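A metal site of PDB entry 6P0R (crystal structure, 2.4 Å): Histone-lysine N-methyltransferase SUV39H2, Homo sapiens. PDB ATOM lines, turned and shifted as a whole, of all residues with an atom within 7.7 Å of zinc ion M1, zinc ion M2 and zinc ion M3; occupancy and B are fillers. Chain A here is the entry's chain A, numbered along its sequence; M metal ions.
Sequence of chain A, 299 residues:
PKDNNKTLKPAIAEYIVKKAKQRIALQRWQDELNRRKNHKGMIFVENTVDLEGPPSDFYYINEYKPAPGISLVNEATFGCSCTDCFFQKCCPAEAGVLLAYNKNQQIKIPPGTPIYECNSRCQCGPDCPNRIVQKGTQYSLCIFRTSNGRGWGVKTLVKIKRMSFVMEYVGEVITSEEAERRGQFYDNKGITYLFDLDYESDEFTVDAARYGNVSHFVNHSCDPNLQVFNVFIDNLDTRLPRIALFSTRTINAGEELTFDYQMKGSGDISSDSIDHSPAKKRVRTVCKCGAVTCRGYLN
NH1 of Arg 131 is in hydrogen-bond range of O of Cys 118 (3.5 Å).
The backbone carbonyl oxygen of Cys 124 sits at hydrogen-bond distance from the guanidinium group of Arg 131 (3.0 Å).
The side-chain sulfur (SG) of Cys 128 sits close to the backbone NH (N) of Asn 130 (3.3 Å).
O of Cys 80 lies within hydrogen-bond range of N of Gln 123.
N of Cys 118 lies within hydrogen-bond range of O of Asn 130 (3.2 Å).
N of Asn 119 sits close to SG of Cys 122 (3.4 Å).
The side-chain sulfur (SG) of Cys 80 binds zinc ion M2, at 2.3 Å.
Zinc ion M2 is bound by the side-chain sulfur (SG) of Cys 82.
Zinc ion M2 is bound by SG of Cys 85, at 2.3 Å.
The side-chain sulfur (SG) of Cys 90 binds zinc ion M2 (2.3 Å).
Zinc ion M2 has four donor atoms within binding distance.
Zinc ion M3 is bound by SG of Cys 80, SG of Cys 91, SG of Cys 122 and SG of Cys 118.
Within 4 Å of zinc ion M2: Cys 80, Cys 82, Cys 85, Cys 90 and Cys 118.
The side-chain sulfur (SG) of Cys 124 binds zinc ion M1 (2.3 Å).
Zinc ion M1 is bound by the side-chain sulfur (SG) of Cys 85, 2.3 Å away.
SG of Cys 118 binds zinc ion M1 (2.3 Å).
SG of Cys 128 binds zinc ion M1 (2.4 Å).
Of the 28 residues printed, 5 come within 4 Å of zinc ion M1.
The nearest printed residue that does not touch zinc ion M1 is Cys 90 (4.3 Å).
Of the 28 residues printed, 5 come within 4 Å of zinc ion M3.
The nearest printed residue that does not touch zinc ion M3 is Cys 124 (4.6 Å).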
ATOM      1  N   PHE A  78       7.054 -11.447 -20.581  1.00  0.00           N
ATOM      2  CA  PHE A  78       8.309 -11.315 -19.835  1.00  0.00           C
ATOM      3  C   PHE A  78       9.013 -12.659 -19.639  1.00  0.00           C
ATOM      4  O   PHE A  78       8.371 -13.691 -19.432  1.00  0.00           O
ATOM      5  CB  PHE A  78       8.066 -10.691 -18.453  1.00  0.00           C
ATOM      6  CG  PHE A  78       7.674  -9.244 -18.510  1.00  0.00           C
ATOM      7  CD1 PHE A  78       8.608  -8.275 -18.874  1.00  0.00           C
ATOM      8  CD2 PHE A  78       6.363  -8.843 -18.210  1.00  0.00           C
ATOM      9  CE1 PHE A  78       8.252  -6.925 -18.943  1.00  0.00           C
ATOM     10  CE2 PHE A  78       6.009  -7.498 -18.263  1.00  0.00           C
ATOM     11  CZ  PHE A  78       6.943  -6.538 -18.625  1.00  0.00           C
ATOM     12  N   GLY A  79      10.338 -12.626 -19.717  1.00  0.00           N
ATOM     13  CA  GLY A  79      11.180 -13.783 -19.450  1.00  0.00           C
ATOM     14  C   GLY A  79      12.219 -13.429 -18.411  1.00  0.00           C
ATOM     15  O   GLY A  79      12.095 -12.411 -17.723  1.00  0.00           O
ATOM     16  N   CYS A  80      13.214 -14.275 -18.286  1.00  0.00           N
ATOM     17  CA  CYS A  80      14.305 -14.060 -17.339  1.00  0.00           C
ATOM     18  C   CYS A  80      15.419 -13.306 -18.000  1.00  0.00           C
ATOM     19  O   CYS A  80      15.419 -13.132 -19.221  1.00  0.00           O
ATOM     20  CB  CYS A  80      14.835 -15.383 -16.833  1.00  0.00           C
ATOM     21  SG  CYS A  80      15.529 -16.471 -18.106  1.00  0.00           S
ATOM     22  N   SER A  81      16.371 -12.850 -17.197  1.00  0.00           N
ATOM     23  CA  SER A  81      17.564 -12.181 -17.671  1.00  0.00           C
ATOM     24  C   SER A  81      18.845 -12.834 -17.102  1.00  0.00           C
ATOM     25  O   SER A  81      19.891 -12.174 -16.990  1.00  0.00           O
ATOM     26  CB  SER A  81      17.539 -10.694 -17.285  1.00  0.00           C
ATOM     27  OG  SER A  81      16.269 -10.113 -17.504  1.00  0.00           O
ATOM     28  N   CYS A  82      18.771 -14.146 -16.757  1.00  0.00           N
ATOM     29  CA  CYS A  82      19.951 -14.880 -16.297  1.00  0.00           C
ATOM     30  C   CYS A  82      21.025 -14.905 -17.382  1.00  0.00           C
ATOM     31  O   CYS A  82      20.707 -14.901 -18.586  1.00  0.00           O
ATOM     32  CB  CYS A  82      19.617 -16.358 -15.930  1.00  0.00           C
ATOM     33  SG  CYS A  82      18.000 -16.696 -15.250  1.00  0.00           S
ATOM     34  N   THR A  83      22.283 -14.946 -16.963  1.00  0.00           N
ATOM     35  CA  THR A  83      23.379 -15.367 -17.838  1.00  0.00           C
ATOM     36  C   THR A  83      23.626 -16.892 -17.706  1.00  0.00           C
ATOM     37  O   THR A  83      24.092 -17.529 -18.653  1.00  0.00           O
ATOM     38  CB  THR A  83      24.670 -14.568 -17.559  1.00  0.00           C
ATOM     39  OG1 THR A  83      25.028 -14.697 -16.188  1.00  0.00           O
ATOM     40  CG2 THR A  83      24.453 -13.096 -17.874  1.00  0.00           C
ATOM     41  N   ASP A  84      23.304 -17.452 -16.519  1.00  0.00           N
ATOM     42  CA  ASP A  84      23.318 -18.911 -16.261  1.00  0.00           C
ATOM     43  C   ASP A  84      21.962 -19.343 -15.665  1.00  0.00           C
ATOM     44  O   ASP A  84      21.734 -19.233 -14.462  1.00  0.00           O
ATOM     45  CB  ASP A  84      24.458 -19.280 -15.281  1.00  0.00           C
ATOM     46  CG  ASP A  84      24.590 -20.806 -15.057  1.00  0.00           C
ATOM     47  OD1 ASP A  84      23.558 -21.536 -15.127  1.00  0.00           O
ATOM     48  OD2 ASP A  84      25.708 -21.277 -14.790  1.00  0.00           O
ATOM     49  N   CYS A  85      21.081 -19.865 -16.525  1.00  0.00           N
ATOM     50  CA  CYS A  85      19.719 -20.212 -16.097  1.00  0.00           C
ATOM     51  C   CYS A  85      19.634 -21.418 -15.155  1.00  0.00           C
ATOM     52  O   CYS A  85      18.606 -21.612 -14.495  1.00  0.00           O
ATOM     53  CB  CYS A  85      18.838 -20.454 -17.313  1.00  0.00           C
ATOM     54  SG  CYS A  85      18.386 -18.957 -18.192  1.00  0.00           S
ATOM     55  N   PHE A  86      20.688 -22.232 -15.109  1.00  0.00           N
ATOM     56  CA  PHE A  86      20.734 -23.372 -14.185  1.00  0.00           C
ATOM     57  C   PHE A  86      20.954 -22.910 -12.738  1.00  0.00           C
ATOM     58  O   PHE A  86      20.259 -23.356 -11.831  1.00  0.00           O
ATOM     59  CB  PHE A  86      21.842 -24.367 -14.606  1.00  0.00           C
ATOM     60  CG  PHE A  86      21.865 -25.627 -13.797  1.00  0.00           C
ATOM     61  CD1 PHE A  86      20.929 -26.638 -14.018  1.00  0.00           C
ATOM     62  CD2 PHE A  86      22.833 -25.814 -12.804  1.00  0.00           C
ATOM     63  CE1 PHE A  86      20.951 -27.800 -13.263  1.00  0.00           C
ATOM     64  CE2 PHE A  86      22.863 -26.983 -12.040  1.00  0.00           C
ATOM     65  CZ  PHE A  86      21.910 -27.979 -12.278  1.00  0.00           C
ATOM     66  N   GLN A  88      20.989 -19.488 -11.603  1.00  0.00           N
ATOM     67  CA  GLN A  88      20.254 -18.280 -11.206  1.00  0.00           C
ATOM     68  C   GLN A  88      18.755 -18.561 -11.018  1.00  0.00           C
ATOM     69  O   GLN A  88      18.212 -19.486 -11.615  1.00  0.00           O
ATOM     70  CB  GLN A  88      20.450 -17.176 -12.230  1.00  0.00           C
ATOM     71  CG  GLN A  88      21.877 -16.702 -12.355  1.00  0.00           C
ATOM     72  CD  GLN A  88      21.995 -15.473 -13.227  1.00  0.00           C
ATOM     73  OE1 GLN A  88      22.519 -15.533 -14.354  1.00  0.00           O
ATOM     74  NE2 GLN A  88      21.489 -14.339 -12.736  1.00  0.00           N
ATOM     75  N   LYS A  89      18.114 -17.747 -10.176  1.00  0.00           N
ATOM     76  CA  LYS A  89      16.657 -17.774 -10.020  1.00  0.00           C
ATOM     77  C   LYS A  89      16.066 -17.331 -11.343  1.00  0.00           C
ATOM     78  O   LYS A  89      16.265 -16.195 -11.779  1.00  0.00           O
ATOM     79  CB  LYS A  89      16.176 -16.868  -8.871  1.00  0.00           C
ATOM     80  CG  LYS A  89      16.283 -17.503  -7.500  1.00  0.00           C
ATOM     81  CD  LYS A  89      16.060 -16.507  -6.379  1.00  0.00           C
ATOM     82  CE  LYS A  89      14.606 -16.037  -6.312  1.00  0.00           C
ATOM     83  NZ  LYS A  89      14.282 -15.416  -4.992  1.00  0.00           N
ATOM     84  N   CYS A  90      15.314 -18.239 -11.952  1.00  0.00           N
ATOM     85  CA  CYS A  90      15.015 -18.191 -13.359  1.00  0.00           C
ATOM     86  C   CYS A  90      13.482 -18.215 -13.522  1.00  0.00           C
ATOM     87  O   CYS A  90      12.750 -17.968 -12.565  1.00  0.00           O
ATOM     88  CB  CYS A  90      15.696 -19.398 -14.018  1.00  0.00           C
ATOM     89  SG  CYS A  90      15.571 -19.550 -15.807  1.00  0.00           S
ATOM     90  N   CYS A  91      13.014 -18.478 -14.748  1.00  0.00           N
ATOM     91  CA  CYS A  91      11.561 -18.571 -15.052  1.00  0.00           C
ATOM     92  C   CYS A  91      10.758 -19.433 -14.044  1.00  0.00           C
ATOM     93  O   CYS A  91       9.719 -18.986 -13.545  1.00  0.00           O
ATOM     94  CB  CYS A  91      11.339 -19.028 -16.515  1.00  0.00           C
ATOM     95  SG  CYS A  91      11.719 -17.755 -17.775  1.00  0.00           S
ATOM     96  N   PRO A  92      11.256 -20.657 -13.691  1.00  0.00           N
ATOM     97  CA  PRO A  92      10.566 -21.503 -12.690  1.00  0.00           C
ATOM     98  C   PRO A  92      10.392 -20.826 -11.320  1.00  0.00           C
ATOM     99  O   PRO A  92       9.285 -20.864 -10.749  1.00  0.00           O
ATOM    100  CB  PRO A  92      11.480 -22.732 -12.569  1.00  0.00           C
ATOM    101  CG  PRO A  92      12.271 -22.761 -13.820  1.00  0.00           C
ATOM    102  CD  PRO A  92      12.465 -21.332 -14.219  1.00  0.00           C
ATOM    103  N   TYR A 116       8.153 -24.991 -16.275  1.00  0.00           N
ATOM    104  CA  TYR A 116       8.185 -23.643 -16.804  1.00  0.00           C
ATOM    105  C   TYR A 116       9.508 -23.430 -17.499  1.00  0.00           C
ATOM    106  O   TYR A 116      10.548 -23.267 -16.850  1.00  0.00           O
ATOM    107  CB  TYR A 116       7.960 -22.608 -15.695  1.00  0.00           C
ATOM    108  CG  TYR A 116       6.495 -22.429 -15.341  1.00  0.00           C
ATOM    109  CD1 TYR A 116       5.877 -23.233 -14.387  1.00  0.00           C
ATOM    110  CD2 TYR A 116       5.722 -21.442 -15.977  1.00  0.00           C
ATOM    111  CE1 TYR A 116       4.536 -23.066 -14.062  1.00  0.00           C
ATOM    112  CE2 TYR A 116       4.380 -21.257 -15.658  1.00  0.00           C
ATOM    113  CZ  TYR A 116       3.783 -22.081 -14.708  1.00  0.00           C
ATOM    114  OH  TYR A 116       2.442 -21.905 -14.386  1.00  0.00           O
ATOM    115  N   GLU A 117       9.472 -23.471 -18.834  1.00  0.00           N
ATOM    116  CA  GLU A 117      10.670 -23.290 -19.643  1.00  0.00           C
ATOM    117  C   GLU A 117      10.852 -21.853 -19.975  1.00  0.00           C
ATOM    118  O   GLU A 117       9.925 -21.050 -19.843  1.00  0.00           O
ATOM    119  CB  GLU A 117      10.601 -24.114 -20.931  1.00  0.00           C
ATOM    120  CG  GLU A 117      10.464 -25.628 -20.686  1.00  0.00           C
ATOM    121  CD  GLU A 117      10.983 -26.485 -21.819  1.00  0.00           C
ATOM    122  OE1 GLU A 117      11.252 -25.970 -22.932  1.00  0.00           O
ATOM    123  OE2 GLU A 117      11.141 -27.704 -21.589  1.00  0.00           O
ATOM    124  N   CYS A 118      12.073 -21.521 -20.393  1.00  0.00           N
ATOM    125  CA  CYS A 118      12.385 -20.221 -20.963  1.00  0.00           C
ATOM    126  C   CYS A 118      11.690 -20.077 -22.290  1.00  0.00           C
ATOM    127  O   CYS A 118      11.374 -21.080 -22.948  1.00  0.00           O
ATOM    128  CB  CYS A 118      13.895 -20.079 -21.132  1.00  0.00           C
ATOM    129  SG  CYS A 118      14.708 -19.883 -19.570  1.00  0.00           S
ATOM    130  N   ASN A 119      11.470 -18.830 -22.691  1.00  0.00           N
ATOM    131  CA  ASN A 119      10.563 -18.495 -23.792  1.00  0.00           C
ATOM    132  C   ASN A 119      11.205 -17.440 -24.716  1.00  0.00           C
ATOM    133  O   ASN A 119      12.380 -17.141 -24.578  1.00  0.00           O
ATOM    134  CB  ASN A 119       9.184 -18.060 -23.231  1.00  0.00           C
ATOM    135  CG  ASN A 119       9.275 -16.898 -22.245  1.00  0.00           C
ATOM    136  OD1 ASN A 119       9.634 -15.795 -22.612  1.00  0.00           O
ATOM    137  ND2 ASN A 119       8.926 -17.161 -20.975  1.00  0.00           N
ATOM    138  N   ARG A 121      10.823 -14.296 -24.802  1.00  0.00           N
ATOM    139  CA  ARG A 121      11.083 -13.045 -24.108  1.00  0.00           C
ATOM    140  C   ARG A 121      12.293 -13.136 -23.158  1.00  0.00           C
ATOM    141  O   ARG A 121      12.725 -12.134 -22.629  1.00  0.00           O
ATOM    142  CB  ARG A 121       9.833 -12.603 -23.307  1.00  0.00           C
ATOM    143  CG  ARG A 121       8.496 -12.723 -24.068  1.00  0.00           C
ATOM    144  CD  ARG A 121       8.058 -11.422 -24.731  1.00  0.00           C
ATOM    145  NE  ARG A 121       9.084 -10.795 -25.555  1.00  0.00           N
ATOM    146  CZ  ARG A 121       9.307 -11.051 -26.855  1.00  0.00           C
ATOM    147  NH1 ARG A 121      10.297 -10.411 -27.491  1.00  0.00           N
ATOM    148  NH2 ARG A 121       8.564 -11.949 -27.535  1.00  0.00           N
ATOM    149  N   CYS A 122      12.821 -14.357 -22.937  1.00  0.00           N
ATOM    150  CA  CYS A 122      14.040 -14.542 -22.124  1.00  0.00           C
ATOM    151  C   CYS A 122      15.258 -14.118 -22.928  1.00  0.00           C
ATOM    152  O   CYS A 122      15.232 -14.166 -24.151  1.00  0.00           O
ATOM    153  CB  CYS A 122      14.199 -15.995 -21.664  1.00  0.00           C
ATOM    154  SG  CYS A 122      12.932 -16.640 -20.544  1.00  0.00           S
ATOM    155  N   GLN A 123      16.323 -13.742 -22.237  1.00  0.00           N
ATOM    156  CA  GLN A 123      17.578 -13.334 -22.893  1.00  0.00           C
ATOM    157  C   GLN A 123      18.434 -14.506 -23.334  1.00  0.00           C
ATOM    158  O   GLN A 123      19.186 -14.403 -24.314  1.00  0.00           O
ATOM    159  CB  GLN A 123      18.406 -12.409 -21.971  1.00  0.00           C
ATOM    160  CG  GLN A 123      17.693 -11.124 -21.564  1.00  0.00           C
ATOM    161  CD  GLN A 123      17.230 -10.312 -22.766  1.00  0.00           C
ATOM    162  OE1 GLN A 123      17.962 -10.165 -23.735  1.00  0.00           O
ATOM    163  NE2 GLN A 123      15.996  -9.810 -22.704  1.00  0.00           N
ATOM    164  N   CYS A 124      18.351 -15.620 -22.608  1.00  0.00           N
ATOM    165  CA  CYS A 124      19.174 -16.799 -22.892  1.00  0.00           C
ATOM    166  C   CYS A 124      18.953 -17.377 -24.310  1.00  0.00           C
ATOM    167  O   CYS A 124      17.826 -17.314 -24.852  1.00  0.00           O
ATOM    168  CB  CYS A 124      18.924 -17.876 -21.839  1.00  0.00           C
ATOM    169  SG  CYS A 124      17.198 -18.437 -21.807  1.00  0.00           S
ATOM    170  N   GLY A 125      20.021 -17.914 -24.905  1.00  0.00           N
ATOM    171  CA  GLY A 125      19.966 -18.559 -26.229  1.00  0.00           C
ATOM    172  C   GLY A 125      19.433 -19.989 -26.184  1.00  0.00           C
ATOM    173  O   GLY A 125      19.027 -20.476 -25.120  1.00  0.00           O
ATOM    174  N   ASP A 127      20.860 -22.908 -26.351  1.00  0.00           N
ATOM    175  CA  ASP A 127      21.657 -23.783 -25.455  1.00  0.00           C
ATOM    176  C   ASP A 127      21.299 -23.722 -23.941  1.00  0.00           C
ATOM    177  O   ASP A 127      21.907 -24.438 -23.141  1.00  0.00           O
ATOM    178  CB  ASP A 127      23.182 -23.548 -25.663  1.00  0.00           C
ATOM    179  CG  ASP A 127      23.570 -22.047 -25.619  1.00  0.00           C
ATOM    180  OD1 ASP A 127      23.023 -21.257 -26.428  1.00  0.00           O
ATOM    181  OD2 ASP A 127      24.446 -21.698 -24.810  1.00  0.00           O
ATOM    182  N   CYS A 128      20.323 -22.878 -23.559  1.00  0.00           N
ATOM    183  CA  CYS A 128      19.815 -22.836 -22.182  1.00  0.00           C
ATOM    184  C   CYS A 128      19.307 -24.214 -21.730  1.00  0.00           C
ATOM    185  O   CYS A 128      18.547 -24.835 -22.457  1.00  0.00           O
ATOM    186  CB  CYS A 128      18.677 -21.796 -22.054  1.00  0.00           C
ATOM    187  SG  CYS A 128      17.795 -21.834 -20.455  1.00  0.00           S
ATOM    188  N   PRO A 129      19.730 -24.685 -20.531  1.00  0.00           N
ATOM    189  CA  PRO A 129      19.297 -26.008 -20.048  1.00  0.00           C
ATOM    190  C   PRO A 129      17.827 -26.085 -19.606  1.00  0.00           C
ATOM    191  O   PRO A 129      17.341 -27.181 -19.365  1.00  0.00           O
ATOM    192  CB  PRO A 129      20.237 -26.273 -18.861  1.00  0.00           C
ATOM    193  CG  PRO A 129      20.596 -24.929 -18.361  1.00  0.00           C
ATOM    194  CD  PRO A 129      20.659 -24.037 -19.575  1.00  0.00           C
ATOM    195  N   ASN A 130      17.144 -24.938 -19.489  1.00  0.00           N
ATOM    196  CA  ASN A 130      15.684 -24.876 -19.346  1.00  0.00           C
ATOM    197  C   ASN A 130      14.933 -24.682 -20.703  1.00  0.00           C
ATOM    198  O   ASN A 130      13.795 -24.221 -20.724  1.00  0.00           O
ATOM    199  CB  ASN A 130      15.303 -23.730 -18.361  1.00  0.00           C
ATOM    200  CG  ASN A 130      13.917 -23.909 -17.750  1.00  0.00           C
ATOM    201  OD1 ASN A 130      13.446 -25.029 -17.556  1.00  0.00           O
ATOM    202  ND2 ASN A 130      13.266 -22.780 -17.423  1.00  0.00           N
ATOM    203  N   ARG A 131      15.591 -25.015 -21.825  1.00  0.00           N
ATOM    204  CA  ARG A 131      14.947 -25.048 -23.156  1.00  0.00           C
ATOM    205  C   ARG A 131      15.048 -26.466 -23.746  1.00  0.00           C
ATOM    206  O   ARG A 131      15.956 -26.755 -24.529  1.00  0.00           O
ATOM    207  CB  ARG A 131      15.600 -24.020 -24.103  1.00  0.00           C
ATOM    208  CG  ARG A 131      15.321 -22.560 -23.791  1.00  0.00           C
ATOM    209  CD  ARG A 131      15.943 -21.684 -24.852  1.00  0.00           C
ATOM    210  NE  ARG A 131      15.889 -20.240 -24.568  1.00  0.00           N
ATOM    211  CZ  ARG A 131      14.841 -19.434 -24.815  1.00  0.00           C
ATOM    212  NH1 ARG A 131      13.689 -19.927 -25.285  1.00  0.00           N
ATOM    213  NH2 ARG A 131      14.942 -18.126 -24.557  1.00  0.00           N
HETATM  214 ZN    ZN M   1      17.002 -19.689 -19.892  1.00  0.00          ZN
HETATM  215 ZN    ZN M   2      16.824 -17.875 -16.842  1.00  0.00          ZN
HETATM  216 ZN    ZN M   3      13.810 -17.858 -18.760  1.00  0.00          ZN
